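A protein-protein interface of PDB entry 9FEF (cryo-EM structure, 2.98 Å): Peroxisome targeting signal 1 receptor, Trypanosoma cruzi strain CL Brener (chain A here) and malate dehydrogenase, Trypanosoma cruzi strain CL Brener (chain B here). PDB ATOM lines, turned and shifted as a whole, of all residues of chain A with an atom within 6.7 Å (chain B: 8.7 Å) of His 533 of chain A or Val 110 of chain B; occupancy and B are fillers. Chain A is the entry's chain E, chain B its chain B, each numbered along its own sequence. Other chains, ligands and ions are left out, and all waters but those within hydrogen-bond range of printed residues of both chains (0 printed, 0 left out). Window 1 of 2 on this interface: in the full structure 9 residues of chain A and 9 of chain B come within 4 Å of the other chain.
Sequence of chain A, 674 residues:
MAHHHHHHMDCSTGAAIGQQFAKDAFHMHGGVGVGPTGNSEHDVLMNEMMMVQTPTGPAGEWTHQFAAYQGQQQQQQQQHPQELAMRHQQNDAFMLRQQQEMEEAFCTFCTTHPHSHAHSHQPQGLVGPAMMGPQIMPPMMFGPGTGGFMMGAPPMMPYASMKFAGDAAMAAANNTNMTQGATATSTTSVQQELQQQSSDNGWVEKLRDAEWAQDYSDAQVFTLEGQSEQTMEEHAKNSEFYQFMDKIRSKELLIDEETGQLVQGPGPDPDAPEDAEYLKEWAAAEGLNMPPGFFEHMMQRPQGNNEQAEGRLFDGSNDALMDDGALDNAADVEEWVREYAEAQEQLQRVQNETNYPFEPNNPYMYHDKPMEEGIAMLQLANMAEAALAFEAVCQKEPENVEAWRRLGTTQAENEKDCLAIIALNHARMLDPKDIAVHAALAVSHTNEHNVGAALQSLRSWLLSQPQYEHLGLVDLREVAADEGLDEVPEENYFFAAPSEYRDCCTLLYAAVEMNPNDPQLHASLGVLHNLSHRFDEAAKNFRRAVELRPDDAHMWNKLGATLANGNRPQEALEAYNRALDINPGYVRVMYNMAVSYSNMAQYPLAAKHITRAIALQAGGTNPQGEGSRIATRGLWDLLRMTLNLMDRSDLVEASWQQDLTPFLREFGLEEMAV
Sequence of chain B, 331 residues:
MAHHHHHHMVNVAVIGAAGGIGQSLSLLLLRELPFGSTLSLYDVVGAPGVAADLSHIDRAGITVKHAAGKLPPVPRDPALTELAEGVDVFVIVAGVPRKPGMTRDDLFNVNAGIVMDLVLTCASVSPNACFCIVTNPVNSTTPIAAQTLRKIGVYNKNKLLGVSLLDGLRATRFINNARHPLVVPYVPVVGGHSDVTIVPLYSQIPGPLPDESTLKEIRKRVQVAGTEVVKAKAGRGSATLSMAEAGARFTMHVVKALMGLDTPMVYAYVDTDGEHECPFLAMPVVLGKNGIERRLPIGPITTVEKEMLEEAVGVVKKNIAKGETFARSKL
Among the printed residues, merely in contact across the chains: Val 451 of chain A with Pro 73 of chain B, His 533 of chain A with Val 110 of chain B and Phe 535 of chain A with Asp 106 of chain B.
His 533 of chain A touches just one residue of chain B: Val 110 (3.7 Å).
Of chain A, only His 533 (3.7 Å) comes within 4 Å of Val 110 of chain B.
No residue of chain B comes within 4 Å of Ser 532 of chain A.
Arg 534 of chain A touches none of the printed residues of chain B.
Printed residues of chain A within 4 Å of Pro 73 of chain B: Val 451 (3.8 Å).
Printed residues of chain A within 4 Å of Asp 106 of chain B: Phe 535 (3.9 Å).
Of the printed residues of chain B, Val 451 of chain A touches Pro 73 (3.8 Å).
The nearest residue of chain B that does not touch His 533 of chain A is Asp 106 of chain B (5.5 Å).
The nearest residue of chain A that does not touch Val 110 of chain B is Phe 535 of chain A (6.4 Å).
The nearest printed residue of chain B that does not touch Val 451 of chain A is Ile 114 of chain B (9.5 Å).
O of Asp 106 of chain B sits close to OD1 of Asn 109 of chain B.
Printed residues of chain A that touch a printed residue of chain B: Val 451, His 533 and Phe 535.
Hydrophobic or aromatic side chains of chain A that line the printed part of chain B: His 533 and Phe 535.
Printed residues of chain B that touch a printed residue of chain A: Pro 73, Asp 106 and Val 110.
Hydrophobic or aromatic side chains of chain B that line the printed part of chain A: Val 110.
Among the printed residues, 3 pairs touch across the chains.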
ATOM      1  N   VAL A 451      33.371 -24.723  14.254  1.00  0.00           N
ATOM      2  CA  VAL A 451      32.899 -25.925  13.573  1.00  0.00           C
ATOM      3  C   VAL A 451      32.900 -25.726  12.061  1.00  0.00           C
ATOM      4  O   VAL A 451      33.327 -26.607  11.304  1.00  0.00           O
ATOM      5  CB  VAL A 451      31.505 -26.322  14.090  1.00  0.00           C
ATOM      6  CG1 VAL A 451      31.090 -27.668  13.515  1.00  0.00           C
ATOM      7  CG2 VAL A 451      31.494 -26.356  15.610  1.00  0.00           C
ATOM      8  N   LEU A 528      36.863 -34.986  13.317  1.00  0.00           N
ATOM      9  CA  LEU A 528      35.466 -34.660  13.048  1.00  0.00           C
ATOM     10  C   LEU A 528      34.562 -35.091  14.197  1.00  0.00           C
ATOM     11  O   LEU A 528      33.592 -34.398  14.526  1.00  0.00           O
ATOM     12  CB  LEU A 528      35.025 -35.314  11.738  1.00  0.00           C
ATOM     13  CG  LEU A 528      33.541 -35.253  11.378  1.00  0.00           C
ATOM     14  CD1 LEU A 528      33.361 -34.750   9.955  1.00  0.00           C
ATOM     15  CD2 LEU A 528      32.893 -36.617  11.554  1.00  0.00           C
ATOM     16  N   HIS A 529      34.850 -36.239  14.810  1.00  0.00           N
ATOM     17  CA  HIS A 529      34.047 -36.703  15.932  1.00  0.00           C
ATOM     18  C   HIS A 529      34.347 -35.950  17.223  1.00  0.00           C
ATOM     19  O   HIS A 529      33.495 -35.919  18.117  1.00  0.00           O
ATOM     20  CB  HIS A 529      34.260 -38.203  16.148  1.00  0.00           C
ATOM     21  CG  HIS A 529      33.347 -39.066  15.335  1.00  0.00           C
ATOM     22  ND1 HIS A 529      31.976 -39.031  15.469  1.00  0.00           N
ATOM     23  CD2 HIS A 529      33.608 -39.989  14.380  1.00  0.00           C
ATOM     24  CE1 HIS A 529      31.432 -39.895  14.630  1.00  0.00           C
ATOM     25  NE2 HIS A 529      32.401 -40.490  13.957  1.00  0.00           N
ATOM     26  N   ASN A 530      35.532 -35.346  17.340  1.00  0.00           N
ATOM     27  CA  ASN A 530      35.890 -34.645  18.570  1.00  0.00           C
ATOM     28  C   ASN A 530      35.045 -33.392  18.764  1.00  0.00           C
ATOM     29  O   ASN A 530      34.487 -33.170  19.844  1.00  0.00           O
ATOM     30  CB  ASN A 530      37.377 -34.290  18.556  1.00  0.00           C
ATOM     31  CG  ASN A 530      38.188 -35.148  19.504  1.00  0.00           C
ATOM     32  OD1 ASN A 530      37.643 -35.769  20.416  1.00  0.00           O
ATOM     33  ND2 ASN A 530      39.498 -35.189  19.292  1.00  0.00           N
ATOM     34  N   LEU A 531      34.935 -32.562  17.727  1.00  0.00           N
ATOM     35  CA  LEU A 531      34.183 -31.320  17.837  1.00  0.00           C
ATOM     36  C   LEU A 531      32.680 -31.524  17.692  1.00  0.00           C
ATOM     37  O   LEU A 531      31.923 -30.563  17.860  1.00  0.00           O
ATOM     38  CB  LEU A 531      34.682 -30.308  16.801  1.00  0.00           C
ATOM     39  CG  LEU A 531      34.030 -30.272  15.419  1.00  0.00           C
ATOM     40  CD1 LEU A 531      34.342 -28.957  14.741  1.00  0.00           C
ATOM     41  CD2 LEU A 531      34.524 -31.421  14.569  1.00  0.00           C
ATOM     42  N   SER A 532      32.235 -32.742  17.393  1.00  0.00           N
ATOM     43  CA  SER A 532      30.820 -33.077  17.359  1.00  0.00           C
ATOM     44  C   SER A 532      30.319 -33.622  18.691  1.00  0.00           C
ATOM     45  O   SER A 532      29.174 -34.079  18.768  1.00  0.00           O
ATOM     46  CB  SER A 532      30.544 -34.090  16.246  1.00  0.00           C
ATOM     47  OG  SER A 532      31.150 -35.338  16.533  1.00  0.00           O
ATOM     48  N   HIS A 533      31.160 -33.601  19.727  1.00  0.00           N
ATOM     49  CA  HIS A 533      30.865 -34.068  21.081  1.00  0.00           C
ATOM     50  C   HIS A 533      30.636 -35.572  21.157  1.00  0.00           C
ATOM     51  O   HIS A 533      30.227 -36.073  22.212  1.00  0.00           O
ATOM     52  CB  HIS A 533      29.662 -33.336  21.692  1.00  0.00           C
ATOM     53  CG  HIS A 533      29.737 -31.845  21.569  1.00  0.00           C
ATOM     54  ND1 HIS A 533      28.963 -31.132  20.680  1.00  0.00           N
ATOM     55  CD2 HIS A 533      30.497 -30.934  22.220  1.00  0.00           C
ATOM     56  CE1 HIS A 533      29.240 -29.846  20.791  1.00  0.00           C
ATOM     57  NE2 HIS A 533      30.169 -29.698  21.719  1.00  0.00           N
ATOM     58  N   ARG A 534      30.890 -36.309  20.075  1.00  0.00           N
ATOM     59  CA  ARG A 534      30.808 -37.770  20.091  1.00  0.00           C
ATOM     60  C   ARG A 534      32.208 -38.317  20.355  1.00  0.00           C
ATOM     61  O   ARG A 534      32.936 -38.735  19.453  1.00  0.00           O
ATOM     62  CB  ARG A 534      30.228 -38.291  18.781  1.00  0.00           C
ATOM     63  CG  ARG A 534      28.718 -38.139  18.655  1.00  0.00           C
ATOM     64  CD  ARG A 534      28.003 -38.493  19.952  1.00  0.00           C
ATOM     65  NE  ARG A 534      27.480 -37.315  20.635  1.00  0.00           N
ATOM     66  CZ  ARG A 534      27.327 -37.215  21.948  1.00  0.00           C
ATOM     67  NH1 ARG A 534      27.644 -38.212  22.759  1.00  0.00           N
ATOM     68  NH2 ARG A 534      26.843 -36.088  22.461  1.00  0.00           N
ATOM     69  N   PHE A 535      32.584 -38.309  21.636  1.00  0.00           N
ATOM     70  CA  PHE A 535      33.946 -38.656  22.024  1.00  0.00           C
ATOM     71  C   PHE A 535      34.253 -40.138  21.855  1.00  0.00           C
ATOM     72  O   PHE A 535      35.422 -40.495  21.678  1.00  0.00           O
ATOM     73  CB  PHE A 535      34.197 -38.235  23.473  1.00  0.00           C
ATOM     74  CG  PHE A 535      33.969 -36.771  23.727  1.00  0.00           C
ATOM     75  CD1 PHE A 535      34.277 -35.829  22.759  1.00  0.00           C
ATOM     76  CD2 PHE A 535      33.439 -36.336  24.930  1.00  0.00           C
ATOM     77  CE1 PHE A 535      34.067 -34.484  22.988  1.00  0.00           C
ATOM     78  CE2 PHE A 535      33.227 -34.991  25.165  1.00  0.00           C
ATOM     79  CZ  PHE A 535      33.541 -34.064  24.193  1.00  0.00           C
ATOM     80  N   ASP A 536      33.241 -41.007  21.901  1.00  0.00           N
ATOM     81  CA  ASP A 536      33.492 -42.442  21.795  1.00  0.00           C
ATOM     82  C   ASP A 536      34.011 -42.817  20.410  1.00  0.00           C
ATOM     83  O   ASP A 536      35.013 -43.533  20.284  1.00  0.00           O
ATOM     84  CB  ASP A 536      32.218 -43.221  22.129  1.00  0.00           C
ATOM     85  CG  ASP A 536      30.976 -42.600  21.519  1.00  0.00           C
ATOM     86  OD1 ASP A 536      31.077 -42.011  20.422  1.00  0.00           O
ATOM     87  OD2 ASP A 536      29.899 -42.695  22.142  1.00  0.00           O
ATOM     88  N   PRO B  73      28.013 -23.485  15.022  1.00  0.00           N
ATOM     89  CA  PRO B  73      28.284 -22.300  15.853  1.00  0.00           C
ATOM     90  C   PRO B  73      29.684 -21.716  15.754  1.00  0.00           C
ATOM     91  O   PRO B  73      30.684 -22.440  15.757  1.00  0.00           O
ATOM     92  CB  PRO B  73      28.012 -22.820  17.268  1.00  0.00           C
ATOM     93  CG  PRO B  73      26.947 -23.837  17.070  1.00  0.00           C
ATOM     94  CD  PRO B  73      27.303 -24.531  15.777  1.00  0.00           C
ATOM     95  N   ALA B  94      20.020 -22.667  27.389  1.00  0.00           N
ATOM     96  CA  ALA B  94      20.515 -23.328  26.190  1.00  0.00           C
ATOM     97  C   ALA B  94      21.425 -24.472  26.602  1.00  0.00           C
ATOM     98  O   ALA B  94      22.144 -24.387  27.599  1.00  0.00           O
ATOM     99  CB  ALA B  94      21.261 -22.350  25.277  1.00  0.00           C
ATOM    100  N   GLY B  95      21.395 -25.536  25.818  1.00  0.00           N
ATOM    101  CA  GLY B  95      22.243 -26.679  26.070  1.00  0.00           C
ATOM    102  C   GLY B  95      21.725 -27.914  25.363  1.00  0.00           C
ATOM    103  O   GLY B  95      20.698 -27.889  24.693  1.00  0.00           O
ATOM    104  N   VAL B  96      22.470 -29.001  25.537  1.00  0.00           N
ATOM    105  CA  VAL B  96      22.170 -30.286  24.913  1.00  0.00           C
ATOM    106  C   VAL B  96      20.902 -30.855  25.542  1.00  0.00           C
ATOM    107  O   VAL B  96      20.648 -30.630  26.735  1.00  0.00           O
ATOM    108  CB  VAL B  96      23.365 -31.248  25.044  1.00  0.00           C
ATOM    109  CG1 VAL B  96      23.418 -31.879  26.429  1.00  0.00           C
ATOM    110  CG2 VAL B  96      23.339 -32.314  23.957  1.00  0.00           C
ATOM    111  N   PRO B  97      20.052 -31.560  24.779  1.00  0.00           N
ATOM    112  CA  PRO B  97      18.892 -32.237  25.370  1.00  0.00           C
ATOM    113  C   PRO B  97      19.294 -33.417  26.251  1.00  0.00           C
ATOM    114  O   PRO B  97      18.422 -34.186  26.654  1.00  0.00           O
ATOM    115  CB  PRO B  97      18.101 -32.714  24.146  1.00  0.00           C
ATOM    116  CG  PRO B  97      19.093 -32.743  23.033  1.00  0.00           C
ATOM    117  CD  PRO B  97      20.011 -31.599  23.307  1.00  0.00           C
ATOM    118  N   ASP B 105      27.978 -37.150  33.261  1.00  0.00           N
ATOM    119  CA  ASP B 105      29.182 -36.355  33.442  1.00  0.00           C
ATOM    120  C   ASP B 105      29.614 -35.616  32.186  1.00  0.00           C
ATOM    121  O   ASP B 105      30.283 -34.584  32.300  1.00  0.00           O
ATOM    122  CB  ASP B 105      30.344 -37.240  33.922  1.00  0.00           C
ATOM    123  CG  ASP B 105      31.554 -36.433  34.349  1.00  0.00           C
ATOM    124  OD1 ASP B 105      31.373 -35.409  35.040  1.00  0.00           O
ATOM    125  OD2 ASP B 105      32.686 -36.822  33.993  1.00  0.00           O
ATOM    126  N   ASP B 106      29.251 -36.103  31.002  1.00  0.00           N
ATOM    127  CA  ASP B 106      29.469 -35.388  29.755  1.00  0.00           C
ATOM    128  C   ASP B 106      28.493 -34.235  29.575  1.00  0.00           C
ATOM    129  O   ASP B 106      28.649 -33.442  28.642  1.00  0.00           O
ATOM    130  CB  ASP B 106      29.357 -36.351  28.568  1.00  0.00           C
ATOM    131  CG  ASP B 106      30.470 -37.377  28.543  1.00  0.00           C
ATOM    132  OD1 ASP B 106      30.957 -37.753  29.631  1.00  0.00           O
ATOM    133  OD2 ASP B 106      30.858 -37.809  27.438  1.00  0.00           O
ATOM    134  N   LEU B 107      27.494 -34.131  30.447  1.00  0.00           N
ATOM    135  CA  LEU B 107      26.477 -33.093  30.388  1.00  0.00           C
ATOM    136  C   LEU B 107      27.002 -31.758  30.901  1.00  0.00           C
ATOM    137  O   LEU B 107      26.342 -30.730  30.725  1.00  0.00           O
ATOM    138  CB  LEU B 107      25.249 -33.551  31.191  1.00  0.00           C
ATOM    139  CG  LEU B 107      23.786 -33.183  30.898  1.00  0.00           C
ATOM    140  CD1 LEU B 107      22.891 -33.807  31.957  1.00  0.00           C
ATOM    141  CD2 LEU B 107      23.515 -31.701  30.832  1.00  0.00           C
ATOM    142  N   PHE B 108      28.194 -31.739  31.493  1.00  0.00           N
ATOM    143  CA  PHE B 108      28.751 -30.533  32.088  1.00  0.00           C
ATOM    144  C   PHE B 108      29.666 -29.760  31.153  1.00  0.00           C
ATOM    145  O   PHE B 108      29.541 -28.540  31.054  1.00  0.00           O
ATOM    146  CB  PHE B 108      29.516 -30.873  33.376  1.00  0.00           C
ATOM    147  CG  PHE B 108      30.387 -29.754  33.870  1.00  0.00           C
ATOM    148  CD1 PHE B 108      29.837 -28.534  34.221  1.00  0.00           C
ATOM    149  CD2 PHE B 108      31.757 -29.916  33.970  1.00  0.00           C
ATOM    150  CE1 PHE B 108      30.635 -27.502  34.666  1.00  0.00           C
ATOM    151  CE2 PHE B 108      32.559 -28.885  34.418  1.00  0.00           C
ATOM    152  CZ  PHE B 108      31.997 -27.678  34.766  1.00  0.00           C
ATOM    153  N   ASN B 109      30.603 -30.428  30.477  1.00  0.00           N
ATOM    154  CA  ASN B 109      31.602 -29.705  29.692  1.00  0.00           C
ATOM    155  C   ASN B 109      30.990 -29.043  28.461  1.00  0.00           C
ATOM    156  O   ASN B 109      31.297 -27.882  28.152  1.00  0.00           O
ATOM    157  CB  ASN B 109      32.734 -30.651  29.296  1.00  0.00           C
ATOM    158  CG  ASN B 109      32.237 -32.041  28.957  1.00  0.00           C
ATOM    159  OD1 ASN B 109      31.561 -32.243  27.949  1.00  0.00           O
ATOM    160  ND2 ASN B 109      32.573 -33.010  29.801  1.00  0.00           N
ATOM    161  N   VAL B 110      30.123 -29.765  27.747  1.00  0.00           N
ATOM    162  CA  VAL B 110      29.472 -29.191  26.575  1.00  0.00           C
ATOM    163  C   VAL B 110      28.608 -28.001  26.973  1.00  0.00           C
ATOM    164  O   VAL B 110      28.581 -26.978  26.280  1.00  0.00           O
ATOM    165  CB  VAL B 110      28.660 -30.270  25.830  1.00  0.00           C
ATOM    166  CG1 VAL B 110      27.704 -30.978  26.772  1.00  0.00           C
ATOM    167  CG2 VAL B 110      27.898 -29.653  24.670  1.00  0.00           C
ATOM    168  N   ASN B 111      27.909 -28.104  28.104  1.00  0.00           N
ATOM    169  CA  ASN B 111      27.071 -27.007  28.567  1.00  0.00           C
ATOM    170  C   ASN B 111      27.884 -25.837  29.097  1.00  0.00           C
ATOM    171  O   ASN B 111      27.445 -24.690  28.981  1.00  0.00           O
ATOM    172  CB  ASN B 111      26.116 -27.506  29.646  1.00  0.00           C
ATOM    173  CG  ASN B 111      24.750 -27.819  29.100  1.00  0.00           C
ATOM    174  OD1 ASN B 111      24.112 -26.973  28.485  1.00  0.00           O
ATOM    175  ND2 ASN B 111      24.296 -29.043  29.307  1.00  0.00           N
ATOM    176  N   ALA B 112      29.051 -26.100  29.679  1.00  0.00           N
ATOM    177  CA  ALA B 112      29.917 -25.053  30.197  1.00  0.00           C
ATOM    178  C   ALA B 112      30.566 -24.243  29.088  1.00  0.00           C
ATOM    179  O   ALA B 112      30.686 -23.018  29.206  1.00  0.00           O
ATOM    180  CB  ALA B 112      30.994 -25.667  31.091  1.00  0.00           C
ATOM    181  N   GLY B 113      30.987 -24.904  28.007  1.00  0.00           N
ATOM    182  CA  GLY B 113      31.582 -24.168  26.902  1.00  0.00           C
ATOM    183  C   GLY B 113      30.627 -23.157  26.294  1.00  0.00           C
ATOM    184  O   GLY B 113      30.978 -21.987  26.093  1.00  0.00           O
ATOM    185  N   ILE B 114      29.393 -23.586  26.016  1.00  0.00           N
ATOM    186  CA  ILE B 114      28.435 -22.681  25.392  1.00  0.00           C
ATOM    187  C   ILE B 114      27.978 -21.607  26.372  1.00  0.00           C
ATOM    188  O   ILE B 114      27.688 -20.481  25.961  1.00  0.00           O
ATOM    189  CB  ILE B 114      27.246 -23.460  24.797  1.00  0.00           C
ATOM    190  CG1 ILE B 114      26.181 -23.748  25.852  1.00  0.00           C
ATOM    191  CG2 ILE B 114      27.721 -24.751  24.151  1.00  0.00           C
ATOM    192  CD1 ILE B 114      25.090 -24.655  25.363  1.00  0.00           C
ATOM    193  N   VAL B 115      27.911 -21.919  27.668  1.00  0.00           N
ATOM    194  CA  VAL B 115      27.556 -20.893  28.647  1.00  0.00           C
ATOM    195  C   VAL B 115      28.638 -19.822  28.709  1.00  0.00           C
ATOM    196  O   VAL B 115      28.341 -18.620  28.738  1.00  0.00           O
ATOM    197  CB  VAL B 115      27.300 -21.529  30.025  1.00  0.00           C
ATOM    198  CG1 VAL B 115      27.503 -20.511  31.130  1.00  0.00           C
ATOM    199  CG2 VAL B 115      25.895 -22.095  30.089  1.00  0.00           C
ATOM    200  N   MET B 116      29.907 -20.237  28.716  1.00  0.00           N
ATOM    201  CA  MET B 116      31.002 -19.275  28.670  1.00  0.00           C
ATOM    202  C   MET B 116      30.905 -18.403  27.428  1.00  0.00           C
ATOM    203  O   MET B 116      31.015 -17.174  27.506  1.00  0.00           O
ATOM    204  CB  MET B 116      32.345 -20.006  28.704  1.00  0.00           C
ATOM    205  CG  MET B 116      32.788 -20.448  30.081  1.00  0.00           C
ATOM    206  SD  MET B 116      34.444 -21.159  30.087  1.00  0.00           S
ATOM    207  CE  MET B 116      35.247 -20.149  28.847  1.00  0.00           C
ATOM    208  N   ASP B 117      30.680 -19.027  26.268  1.00  0.00           N
ATOM    209  CA  ASP B 117      30.597 -18.263  25.026  1.00  0.00           C
ATOM    210  C   ASP B 117      29.437 -17.273  25.053  1.00  0.00           C
ATOM    211  O   ASP B 117      29.595 -16.109  24.663  1.00  0.00           O
ATOM    212  CB  ASP B 117      30.461 -19.215  23.839  1.00  0.00           C
ATOM    213  CG  ASP B 117      30.041 -18.506  22.568  1.00  0.00           C
ATOM    214  OD1 ASP B 117      30.637 -17.457  22.248  1.00  0.00           O
ATOM    215  OD2 ASP B 117      29.117 -19.000  21.888  1.00  0.00           O
ATOM    216  N   THR B 135      20.416 -22.947  32.479  1.00  0.00           N
ATOM    217  CA  THR B 135      21.140 -24.158  31.984  1.00  0.00           C
ATOM    218  C   THR B 135      21.144 -25.195  33.112  1.00  0.00           C
ATOM    219  O   THR B 135      20.778 -24.820  34.217  1.00  0.00           O
ATOM    220  CB  THR B 135      22.483 -23.766  31.350  1.00  0.00           C
ATOM    221  OG1 THR B 135      22.252 -22.706  30.424  1.00  0.00           O
ATOM    222  CG2 THR B 135      23.165 -24.907  30.632  1.00  0.00           C
ATOM    223  N   PRO B 137      23.621 -28.109  34.969  1.00  0.00           N
ATOM    224  CA  PRO B 137      24.443 -28.236  36.182  1.00  0.00           C
ATOM    225  C   PRO B 137      24.427 -26.844  36.831  1.00  0.00           C
ATOM    226  O   PRO B 137      25.326 -26.099  36.578  1.00  0.00           O
ATOM    227  CB  PRO B 137      25.785 -28.749  35.655  1.00  0.00           C
ATOM    228  CG  PRO B 137      25.786 -28.386  34.185  1.00  0.00           C
ATOM    229  CD  PRO B 137      24.339 -28.473  33.748  1.00  0.00           C
ATOM    230  N   THR B 141      27.478 -24.083  36.744  1.00  0.00           N
ATOM    231  CA  THR B 141      27.505 -23.078  35.687  1.00  0.00           C
ATOM    232  C   THR B 141      27.356 -21.650  36.192  1.00  0.00           C
ATOM    233  O   THR B 141      27.813 -20.726  35.512  1.00  0.00           O
ATOM    234  CB  THR B 141      26.411 -23.351  34.647  1.00  0.00           C
ATOM    235  OG1 THR B 141      25.153 -23.542  35.303  1.00  0.00           O
ATOM    236  CG2 THR B 141      26.750 -24.585  33.825  1.00  0.00           C
ATOM    237  N   PHE B 326      37.299 -25.499  35.600  1.00  0.00           N
ATOM    238  CA  PHE B 326      37.041 -25.384  34.171  1.00  0.00           C
ATOM    239  C   PHE B 326      36.107 -24.200  33.936  1.00  0.00           C
ATOM    240  O   PHE B 326      36.559 -23.085  33.679  1.00  0.00           O
ATOM    241  CB  PHE B 326      36.439 -26.687  33.630  1.00  0.00           C
ATOM    242  CG  PHE B 326      35.822 -26.566  32.258  1.00  0.00           C
ATOM    243  CD1 PHE B 326      36.375 -25.742  31.288  1.00  0.00           C
ATOM    244  CD2 PHE B 326      34.692 -27.295  31.936  1.00  0.00           C
ATOM    245  CE1 PHE B 326      35.800 -25.640  30.037  1.00  0.00           C
ATOM    246  CE2 PHE B 326      34.120 -27.199  30.685  1.00  0.00           C
ATOM    247  CZ  PHE B 326      34.674 -26.371  29.735  1.00  0.00           C
